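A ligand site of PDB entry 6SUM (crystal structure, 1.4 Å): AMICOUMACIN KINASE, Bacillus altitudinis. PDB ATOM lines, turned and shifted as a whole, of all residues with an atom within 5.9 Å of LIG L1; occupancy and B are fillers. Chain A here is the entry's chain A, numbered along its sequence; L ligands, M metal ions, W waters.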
ATOM      1  N   ALA A  35      30.941 -20.877  -4.815  1.00  0.00           N
ATOM      2  CA  ALA A  35      30.317 -20.855  -3.506  1.00  0.00           C
ATOM      3  C   ALA A  35      29.893 -22.286  -3.149  1.00  0.00           C
ATOM      4  O   ALA A  35      30.672 -22.989  -2.553  1.00  0.00           O
ATOM      5  CB  ALA A  35      29.163 -19.873  -3.473  1.00  0.00           C
ATOM      6  N   GLU A  36      28.732 -22.748  -3.569  1.00  0.00           N
ATOM      7  CA  GLU A  36      28.249 -24.118  -3.286  1.00  0.00           C
ATOM      8  C   GLU A  36      28.593 -25.085  -4.433  1.00  0.00           C
ATOM      9  O   GLU A  36      28.764 -26.268  -4.222  1.00  0.00           O
ATOM     10  CB  GLU A  36      26.726 -24.083  -3.138  1.00  0.00           C
ATOM     11  CG  GLU A  36      26.076 -25.050  -2.157  1.00  0.00           C
ATOM     12  CD  GLU A  36      26.262 -24.645  -0.678  1.00  0.00           C
ATOM     13  OE1 GLU A  36      27.429 -24.647  -0.226  1.00  0.00           O
ATOM     14  OE2 GLU A  36      25.272 -24.375   0.037  1.00  0.00           O
ATOM     15  N   GLU A 160      18.026 -31.041   5.887  1.00  0.00           N
ATOM     16  CA  GLU A 160      19.144 -30.276   5.345  1.00  0.00           C
ATOM     17  C   GLU A 160      20.479 -30.652   5.975  1.00  0.00           C
ATOM     18  O   GLU A 160      20.668 -30.559   7.190  1.00  0.00           O
ATOM     19  CB  GLU A 160      18.882 -28.790   5.588  1.00  0.00           C
ATOM     20  CG  GLU A 160      20.008 -27.830   5.253  1.00  0.00           C
ATOM     21  CD  GLU A 160      20.568 -27.946   3.838  1.00  0.00           C
ATOM     22  OE1 GLU A 160      19.785 -27.765   2.861  1.00  0.00           O
ATOM     23  OE2 GLU A 160      21.817 -28.118   3.740  1.00  0.00           O
ATOM     24  N   GLN A 162      23.323 -29.080   6.062  1.00  0.00           N
ATOM     25  CA  GLN A 162      24.066 -28.046   6.787  1.00  0.00           C
ATOM     26  C   GLN A 162      23.486 -27.734   8.155  1.00  0.00           C
ATOM     27  O   GLN A 162      24.111 -27.013   8.913  1.00  0.00           O
ATOM     28  CB  GLN A 162      24.208 -26.804   5.908  1.00  0.00           C
ATOM     29  CG  GLN A 162      25.146 -27.076   4.717  1.00  0.00           C
ATOM     30  CD  GLN A 162      24.971 -26.102   3.583  1.00  0.00           C
ATOM     31  OE1 GLN A 162      23.967 -25.392   3.505  1.00  0.00           O
ATOM     32  NE2 GLN A 162      25.950 -26.043   2.707  1.00  0.00           N
ATOM     33  N   ALA A 202      13.831 -21.826  -1.544  1.00  0.00           N
ATOM     34  CA  ALA A 202      14.603 -22.001  -0.292  1.00  0.00           C
ATOM     35  C   ALA A 202      15.967 -21.330  -0.264  1.00  0.00           C
ATOM     36  O   ALA A 202      16.733 -21.544   0.667  1.00  0.00           O
ATOM     37  CB  ALA A 202      14.723 -23.462   0.125  1.00  0.00           C
ATOM     38  N   ASP A 203      16.260 -20.466  -1.227  1.00  0.00           N
ATOM     39  CA  ASP A 203      17.463 -19.634  -1.177  1.00  0.00           C
ATOM     40  C   ASP A 203      17.287 -18.353  -1.979  1.00  0.00           C
ATOM     41  O   ASP A 203      18.149 -17.954  -2.758  1.00  0.00           O
ATOM     42  CB  ASP A 203      18.721 -20.382  -1.619  1.00  0.00           C
ATOM     43  CG  ASP A 203      19.987 -19.644  -1.271  1.00  0.00           C
ATOM     44  OD1 ASP A 203      19.991 -18.904  -0.251  1.00  0.00           O
ATOM     45  OD2 ASP A 203      21.001 -19.757  -1.998  1.00  0.00           O
ATOM     46  N   HIS A 205      17.630 -14.780  -2.922  1.00  0.00           N
ATOM     47  CA  HIS A 205      18.499 -13.645  -2.674  1.00  0.00           C
ATOM     48  C   HIS A 205      18.859 -13.030  -4.027  1.00  0.00           C
ATOM     49  O   HIS A 205      18.644 -13.665  -5.055  1.00  0.00           O
ATOM     50  CB  HIS A 205      19.755 -13.983  -1.855  1.00  0.00           C
ATOM     51  CG  HIS A 205      20.722 -14.945  -2.462  1.00  0.00           C
ATOM     52  ND1 HIS A 205      21.518 -14.623  -3.544  1.00  0.00           N
ATOM     53  CD2 HIS A 205      21.174 -16.146  -2.020  1.00  0.00           C
ATOM     54  CE1 HIS A 205      22.335 -15.618  -3.800  1.00  0.00           C
ATOM     55  NE2 HIS A 205      22.163 -16.553  -2.880  1.00  0.00           N
ATOM     56  N   HIS A 206      19.453 -11.840  -3.993  1.00  0.00           N
ATOM     57  CA  HIS A 206      19.673 -11.062  -5.222  1.00  0.00           C
ATOM     58  C   HIS A 206      20.919 -11.448  -5.966  1.00  0.00           C
ATOM     59  O   HIS A 206      21.236 -10.815  -6.964  1.00  0.00           O
ATOM     60  CB  HIS A 206      19.585  -9.561  -4.964  1.00  0.00           C
ATOM     61  CG  HIS A 206      20.347  -9.086  -3.789  1.00  0.00           C
ATOM     62  ND1 HIS A 206      19.937  -9.351  -2.496  1.00  0.00           N
ATOM     63  CD2 HIS A 206      21.482  -8.356  -3.690  1.00  0.00           C
ATOM     64  CE1 HIS A 206      20.780  -8.799  -1.657  1.00  0.00           C
ATOM     65  NE2 HIS A 206      21.739  -8.192  -2.346  1.00  0.00           N
ATOM     66  N   GLY A 207      21.649 -12.460  -5.524  1.00  0.00           N
ATOM     67  CA  GLY A 207      22.561 -13.195  -6.401  1.00  0.00           C
ATOM     68  C   GLY A 207      21.912 -14.309  -7.196  1.00  0.00           C
ATOM     69  O   GLY A 207      22.562 -14.891  -8.071  1.00  0.00           O
ATOM     70  N   ASN A 208      20.625 -14.584  -6.916  1.00  0.00           N
ATOM     71  CA  ASN A 208      19.898 -15.712  -7.490  1.00  0.00           C
ATOM     72  C   ASN A 208      18.737 -15.343  -8.395  1.00  0.00           C
ATOM     73  O   ASN A 208      17.904 -16.185  -8.712  1.00  0.00           O
ATOM     74  CB  ASN A 208      19.404 -16.653  -6.370  1.00  0.00           C
ATOM     75  CG  ASN A 208      20.516 -17.476  -5.767  1.00  0.00           C
ATOM     76  OD1 ASN A 208      21.667 -17.509  -6.271  1.00  0.00           O
ATOM     77  ND2 ASN A 208      20.212 -18.124  -4.638  1.00  0.00           N
ATOM     78  N   ASP A 220      19.249 -20.710  -9.627  1.00  0.00           N
ATOM     79  CA  ASP A 220      19.811 -21.336  -8.433  1.00  0.00           C
ATOM     80  C   ASP A 220      18.720 -21.953  -7.557  1.00  0.00           C
ATOM     81  O   ASP A 220      18.592 -21.620  -6.378  1.00  0.00           O
ATOM     82  CB  ASP A 220      20.704 -20.389  -7.639  1.00  0.00           C
ATOM     83  CG  ASP A 220      21.540 -21.105  -6.602  1.00  0.00           C
ATOM     84  OD1 ASP A 220      21.569 -22.379  -6.532  1.00  0.00           O
ATOM     85  OD2 ASP A 220      22.251 -20.394  -5.815  1.00  0.00           O
ATOM     86  N   ASP A 223      18.873 -25.617  -3.957  1.00  0.00           N
ATOM     87  CA  ASP A 223      18.486 -25.942  -2.572  1.00  0.00           C
ATOM     88  C   ASP A 223      16.990 -26.076  -2.367  1.00  0.00           C
ATOM     89  O   ASP A 223      16.524 -26.177  -1.230  1.00  0.00           O
ATOM     90  CB  ASP A 223      19.116 -24.955  -1.592  1.00  0.00           C
ATOM     91  CG  ASP A 223      20.603 -25.102  -1.564  1.00  0.00           C
ATOM     92  OD1 ASP A 223      21.082 -26.209  -1.205  1.00  0.00           O
ATOM     93  OD2 ASP A 223      21.302 -24.132  -1.946  1.00  0.00           O
ATOM     94  N   ASN A 239      18.682 -12.815   3.813  1.00  0.00           N
ATOM     95  CA  ASN A 239      19.655 -12.509   2.802  1.00  0.00           C
ATOM     96  C   ASN A 239      19.731 -11.014   2.451  1.00  0.00           C
ATOM     97  O   ASN A 239      20.842 -10.493   2.244  1.00  0.00           O
ATOM     98  CB  ASN A 239      19.404 -13.382   1.580  1.00  0.00           C
ATOM     99  CG  ASN A 239      19.833 -14.817   1.800  1.00  0.00           C
ATOM    100  OD1 ASN A 239      20.758 -15.070   2.592  1.00  0.00           O
ATOM    101  ND2 ASN A 239      19.142 -15.774   1.129  1.00  0.00           N
ATOM    102  N   VAL A 240      18.589 -10.327   2.397  1.00  0.00           N
ATOM    103  CA  VAL A 240      18.620  -8.884   2.135  1.00  0.00           C
ATOM    104  C   VAL A 240      19.148  -8.090   3.326  1.00  0.00           C
ATOM    105  O   VAL A 240      19.744  -7.047   3.149  1.00  0.00           O
ATOM    106  CB  VAL A 240      17.294  -8.316   1.614  1.00  0.00           C
ATOM    107  CG1 VAL A 240      16.860  -9.068   0.379  1.00  0.00           C
ATOM    108  CG2 VAL A 240      16.201  -8.291   2.634  1.00  0.00           C
ATOM    109  N   TRP A 242      21.559  -9.278   5.236  1.00  0.00           N
ATOM    110  CA  TRP A 242      22.985  -9.619   5.298  1.00  0.00           C
ATOM    111  C   TRP A 242      23.792  -8.808   4.286  1.00  0.00           C
ATOM    112  O   TRP A 242      24.794  -8.216   4.639  1.00  0.00           O
ATOM    113  CB  TRP A 242      23.139 -11.110   5.052  1.00  0.00           C
ATOM    114  CG  TRP A 242      24.450 -11.725   5.324  1.00  0.00           C
ATOM    115  CD1 TRP A 242      25.567 -11.136   5.903  1.00  0.00           C
ATOM    116  CD2 TRP A 242      24.814 -13.066   5.039  1.00  0.00           C
ATOM    117  NE1 TRP A 242      26.581 -12.047   5.993  1.00  0.00           N
ATOM    118  CE2 TRP A 242      26.158 -13.238   5.445  1.00  0.00           C
ATOM    119  CE3 TRP A 242      24.142 -14.163   4.457  1.00  0.00           C
ATOM    120  CZ2 TRP A 242      26.813 -14.448   5.331  1.00  0.00           C
ATOM    121  CZ3 TRP A 242      24.799 -15.354   4.327  1.00  0.00           C
ATOM    122  CH2 TRP A 242      26.140 -15.490   4.753  1.00  0.00           C
ATOM    123  N   TYR A 243      23.337  -8.801   3.023  1.00  0.00           N
ATOM    124  CA  TYR A 243      24.043  -8.139   1.917  1.00  0.00           C
ATOM    125  C   TYR A 243      23.113  -7.197   1.162  1.00  0.00           C
ATOM    126  O   TYR A 243      22.823  -7.413   0.011  1.00  0.00           O
ATOM    127  CB  TYR A 243      24.682  -9.173   0.967  1.00  0.00           C
ATOM    128  CG  TYR A 243      25.813  -9.961   1.592  1.00  0.00           C
ATOM    129  CD1 TYR A 243      27.026  -9.356   1.906  1.00  0.00           C
ATOM    130  CD2 TYR A 243      25.682 -11.326   1.867  1.00  0.00           C
ATOM    131  CE1 TYR A 243      28.078 -10.079   2.467  1.00  0.00           C
ATOM    132  CE2 TYR A 243      26.732 -12.062   2.410  1.00  0.00           C
ATOM    133  CZ  TYR A 243      27.917 -11.436   2.723  1.00  0.00           C
ATOM    134  OH  TYR A 243      28.938 -12.161   3.284  1.00  0.00           O
ATOM    135  N   ARG A 287      18.115 -20.030  10.005  1.00  0.00           N
ATOM    136  CA  ARG A 287      19.021 -19.747   8.902  1.00  0.00           C
ATOM    137  C   ARG A 287      20.437 -19.426   9.401  1.00  0.00           C
ATOM    138  O   ARG A 287      21.433 -19.823   8.811  1.00  0.00           O
ATOM    139  CB  ARG A 287      18.434 -18.632   8.001  1.00  0.00           C
ATOM    140  CG  ARG A 287      19.175 -18.435   6.683  1.00  0.00           C
ATOM    141  CD  ARG A 287      19.310 -19.721   5.921  1.00  0.00           C
ATOM    142  NE  ARG A 287      19.475 -19.611   4.486  1.00  0.00           N
ATOM    143  CZ  ARG A 287      19.049 -20.505   3.610  1.00  0.00           C
ATOM    144  NH1 ARG A 287      18.320 -21.549   3.978  1.00  0.00           N
ATOM    145  NH2 ARG A 287      19.336 -20.346   2.327  1.00  0.00           N
ATOM    146  N   LEU A 290      22.034 -22.633  10.125  1.00  0.00           N
ATOM    147  CA  LEU A 290      22.386 -23.299   8.890  1.00  0.00           C
ATOM    148  C   LEU A 290      23.682 -22.709   8.334  1.00  0.00           C
ATOM    149  O   LEU A 290      24.569 -23.457   7.910  1.00  0.00           O
ATOM    150  CB  LEU A 290      21.238 -23.168   7.878  1.00  0.00           C
ATOM    151  CG  LEU A 290      21.327 -23.942   6.581  1.00  0.00           C
ATOM    152  CD1 LEU A 290      19.949 -24.227   6.022  1.00  0.00           C
ATOM    153  CD2 LEU A 290      22.196 -23.231   5.550  1.00  0.00           C
ATOM    154  N   ILE A 291      23.809 -21.394   8.313  1.00  0.00           N
ATOM    155  CA  ILE A 291      25.010 -20.746   7.806  1.00  0.00           C
ATOM    156  C   ILE A 291      26.208 -21.191   8.667  1.00  0.00           C
ATOM    157  O   ILE A 291      27.309 -21.444   8.142  1.00  0.00           O
ATOM    158  CB  ILE A 291      24.926 -19.195   7.810  1.00  0.00           C
ATOM    159  CG1 ILE A 291      23.773 -18.684   6.939  1.00  0.00           C
ATOM    160  CG2 ILE A 291      26.214 -18.585   7.280  1.00  0.00           C
ATOM    161  CD1 ILE A 291      23.867 -19.107   5.485  1.00  0.00           C
ATOM    162  N   LEU A 294      27.132 -24.466   7.310  1.00  0.00           N
ATOM    163  CA  LEU A 294      27.773 -24.254   5.995  1.00  0.00           C
ATOM    164  C   LEU A 294      29.226 -23.809   6.131  1.00  0.00           C
ATOM    165  O   LEU A 294      30.126 -24.331   5.445  1.00  0.00           O
ATOM    166  CB  LEU A 294      26.934 -23.266   5.189  1.00  0.00           C
ATOM    167  CG  LEU A 294      27.393 -22.887   3.800  1.00  0.00           C
ATOM    168  CD1 LEU A 294      26.206 -22.325   2.996  1.00  0.00           C
ATOM    169  CD2 LEU A 294      28.561 -21.910   3.748  1.00  0.00           C
ATOM    170  N   LEU A 295      29.478 -22.865   7.039  1.00  0.00           N
ATOM    171  CA  LEU A 295      30.844 -22.353   7.188  1.00  0.00           C
ATOM    172  C   LEU A 295      31.771 -23.445   7.718  1.00  0.00           C
ATOM    173  O   LEU A 295      32.916 -23.548   7.277  1.00  0.00           O
ATOM    174  CB  LEU A 295      30.883 -21.119   8.087  1.00  0.00           C
ATOM    175  CG  LEU A 295      30.114 -19.912   7.534  1.00  0.00           C
ATOM    176  CD1 LEU A 295      30.025 -18.860   8.600  1.00  0.00           C
ATOM    177  CD2 LEU A 295      30.726 -19.338   6.265  1.00  0.00           C
HETATM  178  C1  LIG L   1      23.984 -15.044   0.457  1.00  0.00           C
HETATM  179  C2  LIG L   1      23.614 -13.801  -0.339  1.00  0.00           C
HETATM  180  C3  LIG L   1      22.720 -12.863   0.175  1.00  0.00           C
HETATM  181  C4  LIG L   1      22.398 -11.744  -0.599  1.00  0.00           C
HETATM  182  C5  LIG L   1      22.976 -11.554  -1.860  1.00  0.00           C
HETATM  183  C6  LIG L   1      23.858 -12.497  -2.347  1.00  0.00           C
HETATM  184  O1  LIG L   1      24.400 -12.341  -3.574  1.00  0.00           O
HETATM  185  C7  LIG L   1      24.182 -13.605  -1.593  1.00  0.00           C
HETATM  186  C8  LIG L   1      25.114 -14.635  -2.124  1.00  0.00           C
HETATM  187  O2  LIG L   1      25.486 -14.715  -3.254  1.00  0.00           O
HETATM  188  O3  LIG L   1      25.569 -15.659  -1.299  1.00  0.00           O
HETATM  189  C9  LIG L   1      25.408 -15.459   0.116  1.00  0.00           C
HETATM  190  C10 LIG L   1      25.812 -16.768   0.766  1.00  0.00           C
HETATM  191  C11 LIG L   1      27.252 -17.137   0.406  1.00  0.00           C
HETATM  192  C12 LIG L   1      27.811 -18.339   1.152  1.00  0.00           C
HETATM  193  C13 LIG L   1      29.272 -18.462   0.742  1.00  0.00           C
HETATM  194  C14 LIG L   1      27.700 -18.268   2.659  1.00  0.00           C
HETATM  195  N1  LIG L   1      24.888 -17.848   0.352  1.00  0.00           N
HETATM  196  C15 LIG L   1      23.995 -18.368   1.180  1.00  0.00           C
HETATM  197  O4  LIG L   1      23.896 -18.045   2.340  1.00  0.00           O
HETATM  198  C16 LIG L   1      23.071 -19.435   0.639  1.00  0.00           C
HETATM  199  O5  LIG L   1      23.280 -19.602  -0.767  1.00  0.00           O
HETATM  200  C17 LIG L   1      23.332 -20.773   1.325  1.00  0.00           C
HETATM  201  O6  LIG L   1      23.064 -20.587   2.731  1.00  0.00           O
HETATM  202  C18 LIG L   1      22.427 -21.880   0.816  1.00  0.00           C
HETATM  203  N2  LIG L   1      22.951 -22.369  -0.488  1.00  0.00           N
HETATM  204  C19 LIG L   1      22.428 -23.021   1.818  1.00  0.00           C
HETATM  205  C20 LIG L   1      21.299 -23.981   1.595  1.00  0.00           C
HETATM  206  O7  LIG L   1      20.289 -23.650   1.003  1.00  0.00           O
HETATM  207  N3  LIG L   1      21.444 -25.173   2.129  1.00  0.00           N
HETATM  208  P1  LG2 L   2      24.714 -19.836  -3.762  1.00  0.00           P
HETATM  209  O1  LG2 L   2      23.771 -18.652  -4.067  1.00  0.00           O
HETATM  210  O2  LG2 L   2      24.004 -21.118  -3.417  1.00  0.00           O
HETATM  211  O3  LG2 L   2      25.764 -19.379  -2.748  1.00  0.00           O
HETATM  212  P2  LG2 L   2      25.679 -21.458  -6.172  1.00  0.00           P
HETATM  213  O4  LG2 L   2      27.034 -22.089  -6.050  1.00  0.00           O
HETATM  214  O5  LG2 L   2      24.503 -22.320  -5.958  1.00  0.00           O
HETATM  215  N1  LG2 L   2      25.548 -20.058  -5.244  1.00  0.00           N
HETATM  216  P3  LG2 L   2      24.595 -20.007  -8.521  1.00  0.00           P
HETATM  217  O6  LG2 L   2      23.618 -20.906  -9.204  1.00  0.00           O
HETATM  218  O7  LG2 L   2      24.068 -18.884  -7.696  1.00  0.00           O
HETATM  219  O8  LG2 L   2      25.663 -20.856  -7.670  1.00  0.00           O
HETATM  220  O9  LG2 L   2      25.558 -19.424  -9.661  1.00  0.00           O
HETATM  221  C1  LG2 L   2      26.575 -18.482  -9.399  1.00  0.00           C
HETATM  222  C2  LG2 L   2      26.370 -17.179 -10.139  1.00  0.00           C
HETATM  223  O10 LG2 L   2      26.328 -17.474 -11.551  1.00  0.00           O
HETATM  224  C3  LG2 L   2      25.072 -16.442  -9.867  1.00  0.00           C
HETATM  225  O11 LG2 L   2      25.127 -15.612  -8.715  1.00  0.00           O
HETATM  226  C4  LG2 L   2      24.895 -15.651 -11.146  1.00  0.00           C
HETATM  227  O12 LG2 L   2      25.729 -14.489 -11.159  1.00  0.00           O
HETATM  228  C5  LG2 L   2      25.373 -16.632 -12.190  1.00  0.00           C
HETATM  229  N2  LG2 L   2      24.293 -17.478 -12.714  1.00  0.00           N
HETATM  230  C6  LG2 L   2      23.916 -18.699 -12.254  1.00  0.00           C
HETATM  231  N3  LG2 L   2      22.897 -19.197 -12.963  1.00  0.00           N
HETATM  232  C7  LG2 L   2      22.596 -18.253 -13.874  1.00  0.00           C
HETATM  233  C8  LG2 L   2      21.649 -18.168 -14.963  1.00  0.00           C
HETATM  234  N4  LG2 L   2      20.825 -19.183 -15.216  1.00  0.00           N
HETATM  235  N5  LG2 L   2      21.650 -17.043 -15.731  1.00  0.00           N
HETATM  236  C9  LG2 L   2      22.521 -16.045 -15.483  1.00  0.00           C
HETATM  237  N6  LG2 L   2      23.448 -16.075 -14.514  1.00  0.00           N
HETATM  238  C10 LG2 L   2      23.501 -17.151 -13.708  1.00  0.00           C
HETATM  239 MG    MG M   1      22.896 -22.133  -4.734  1.00  0.00          MG
HETATM  240 MG    MG M   2      23.333 -18.612  -5.964  1.00  0.00          MG
HETATM  241  O   HOH W   1      21.106 -17.712   3.098  1.00  0.00           O
HETATM  242  O   HOH W   2      26.982 -17.131  -3.575  1.00  0.00           O
HETATM  243  O   HOH W   3      24.963  -9.633  -4.110  1.00  0.00           O
HETATM  244  O   HOH W   4      26.564 -20.869  -0.610  1.00  0.00           O
HETATM  245  O   HOH W   5      17.809 -23.657   2.040  1.00  0.00           O
HETATM  246  O   HOH W   6      26.146 -13.762  -5.983  1.00  0.00           O
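An oxygen (O5) of LIG L1 sits at hydrogen-bond distance from an oxygen (O3) of LG2 L2 (3.2 Å).
The side-chain carboxylate (OD2) of Asp 203 lies within salt-bridge range of a nitrogen (N2) of LIG L1.
OD2 of Asp 223 lies within salt-bridge range of N2 of LIG L1, at 2.8 Å.
The side-chain amide oxygen (OE1) of Gln 162 is in hydrogen-bond range of a nitrogen (N3) of LIG L1 (2.9 Å).
The side-chain carboxylate (OE2) of Glu 36 lies within salt-bridge range of a nitrogen (N2) of LIG L1, at 3.1 Å.
The side-chain carboxylate (OE1) of Glu 160 is in hydrogen-bond range of a nitrogen (N3) of LIG L1 (3.2 Å).
N of Gly 207 lies within hydrogen-bond range of O1 of LIG L1.
An oxygen (O4) of LG2 L2 sits at hydrogen-bond distance from the backbone NH (N) of Glu 36.
A ring nitrogen (NE2) of His 205 sits close to an oxygen (O1) of LG2 L2, at 2.9 Å.
O of Gly 207 sits at hydrogen-bond distance from O11 of LG2 L2, 2.7 Å away.
Water W5 lies within hydrogen-bond range of an oxygen (O7) of LIG L1, the backbone carbonyl oxygen of Ala 202 and the guanidinium group of Arg 287.
Water W2 bridges O3 of LG2 L2 (2.7 Å) and O2 of LIG L1 (2.9 Å).
Water W1 lies within hydrogen-bond range of OD1 of Asn 239 (2.7 Å), NE of Arg 287 (2.9 Å) and O4 of LIG L1 (2.9 Å).
Water W6 bridges O2 of LIG L1 (3.0 Å) and O11 of LG2 L2 (3.5 Å).
OD1 of Asp 203 is in salt-bridge range of NH2 of Arg 287.
The backbone carbonyl oxygen of Asp 203 sits at hydrogen-bond distance from the side-chain amide nitrogen of Asn 208 (2.8 Å).
OE2 of Glu 36 is in hydrogen-bond range of NE2 of Gln 162 (3.2 Å).
N of Gln 162 is in hydrogen-bond range of OE2 of Glu 160 (2.9 Å).
The backbone NH (N) of Gly 207 is in hydrogen-bond range of a ring nitrogen (ND1) of His 205, at 2.9 Å.
The side-chain amide nitrogen of Asn 208 sits at hydrogen-bond distance from a ring nitrogen (NE2) of His 205 (3.1 Å).
A ring nitrogen (NE2) of His 206 lies within hydrogen-bond range of the backbone carbonyl oxygen (O) of Tyr 243, 2.7 Å away.
The backbone carbonyl oxygen (O) of Ala 202 lies within hydrogen-bond range of the guanidinium group (NH2) of Arg 287.
His 205 touches LIG L1.
CE1 of His 206 touches C4 of LIG L1 (3.5 Å).
Asn 239 touches LIG L1 (O to C4, 3.5 Å).
Trp 242 touches LIG L1.
CD2 of Tyr 243 touches C3 of LIG L1 (3.7 Å).
Arg 287 touches LIG L1.
CD2 of Leu 290 touches C19 of LIG L1 (3.7 Å).
CD1 of Ile 291 touches O6 of LIG L1, 3.2 Å away.
CD1 of Leu 294 touches O6 of LIG L1 (3.6 Å).
Hydrophobic or aromatic side chains that line LIG L1: His 205, His 206, Trp 242, Tyr 243, Leu 290, Ile 291 and Leu 294.
15 residues have an atom within 4 Å of LIG L1: Glu 36, Glu 160, Gln 162, Asp 203, His 205, His 206, Gly 207, Asp 223, Asn 239, Trp 242, Tyr 243, Arg 287, Leu 290, Ile 291 and Leu 294.
The nearest printed residue that does not touch LIG L1 is Ala 202 (4.1 Å).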
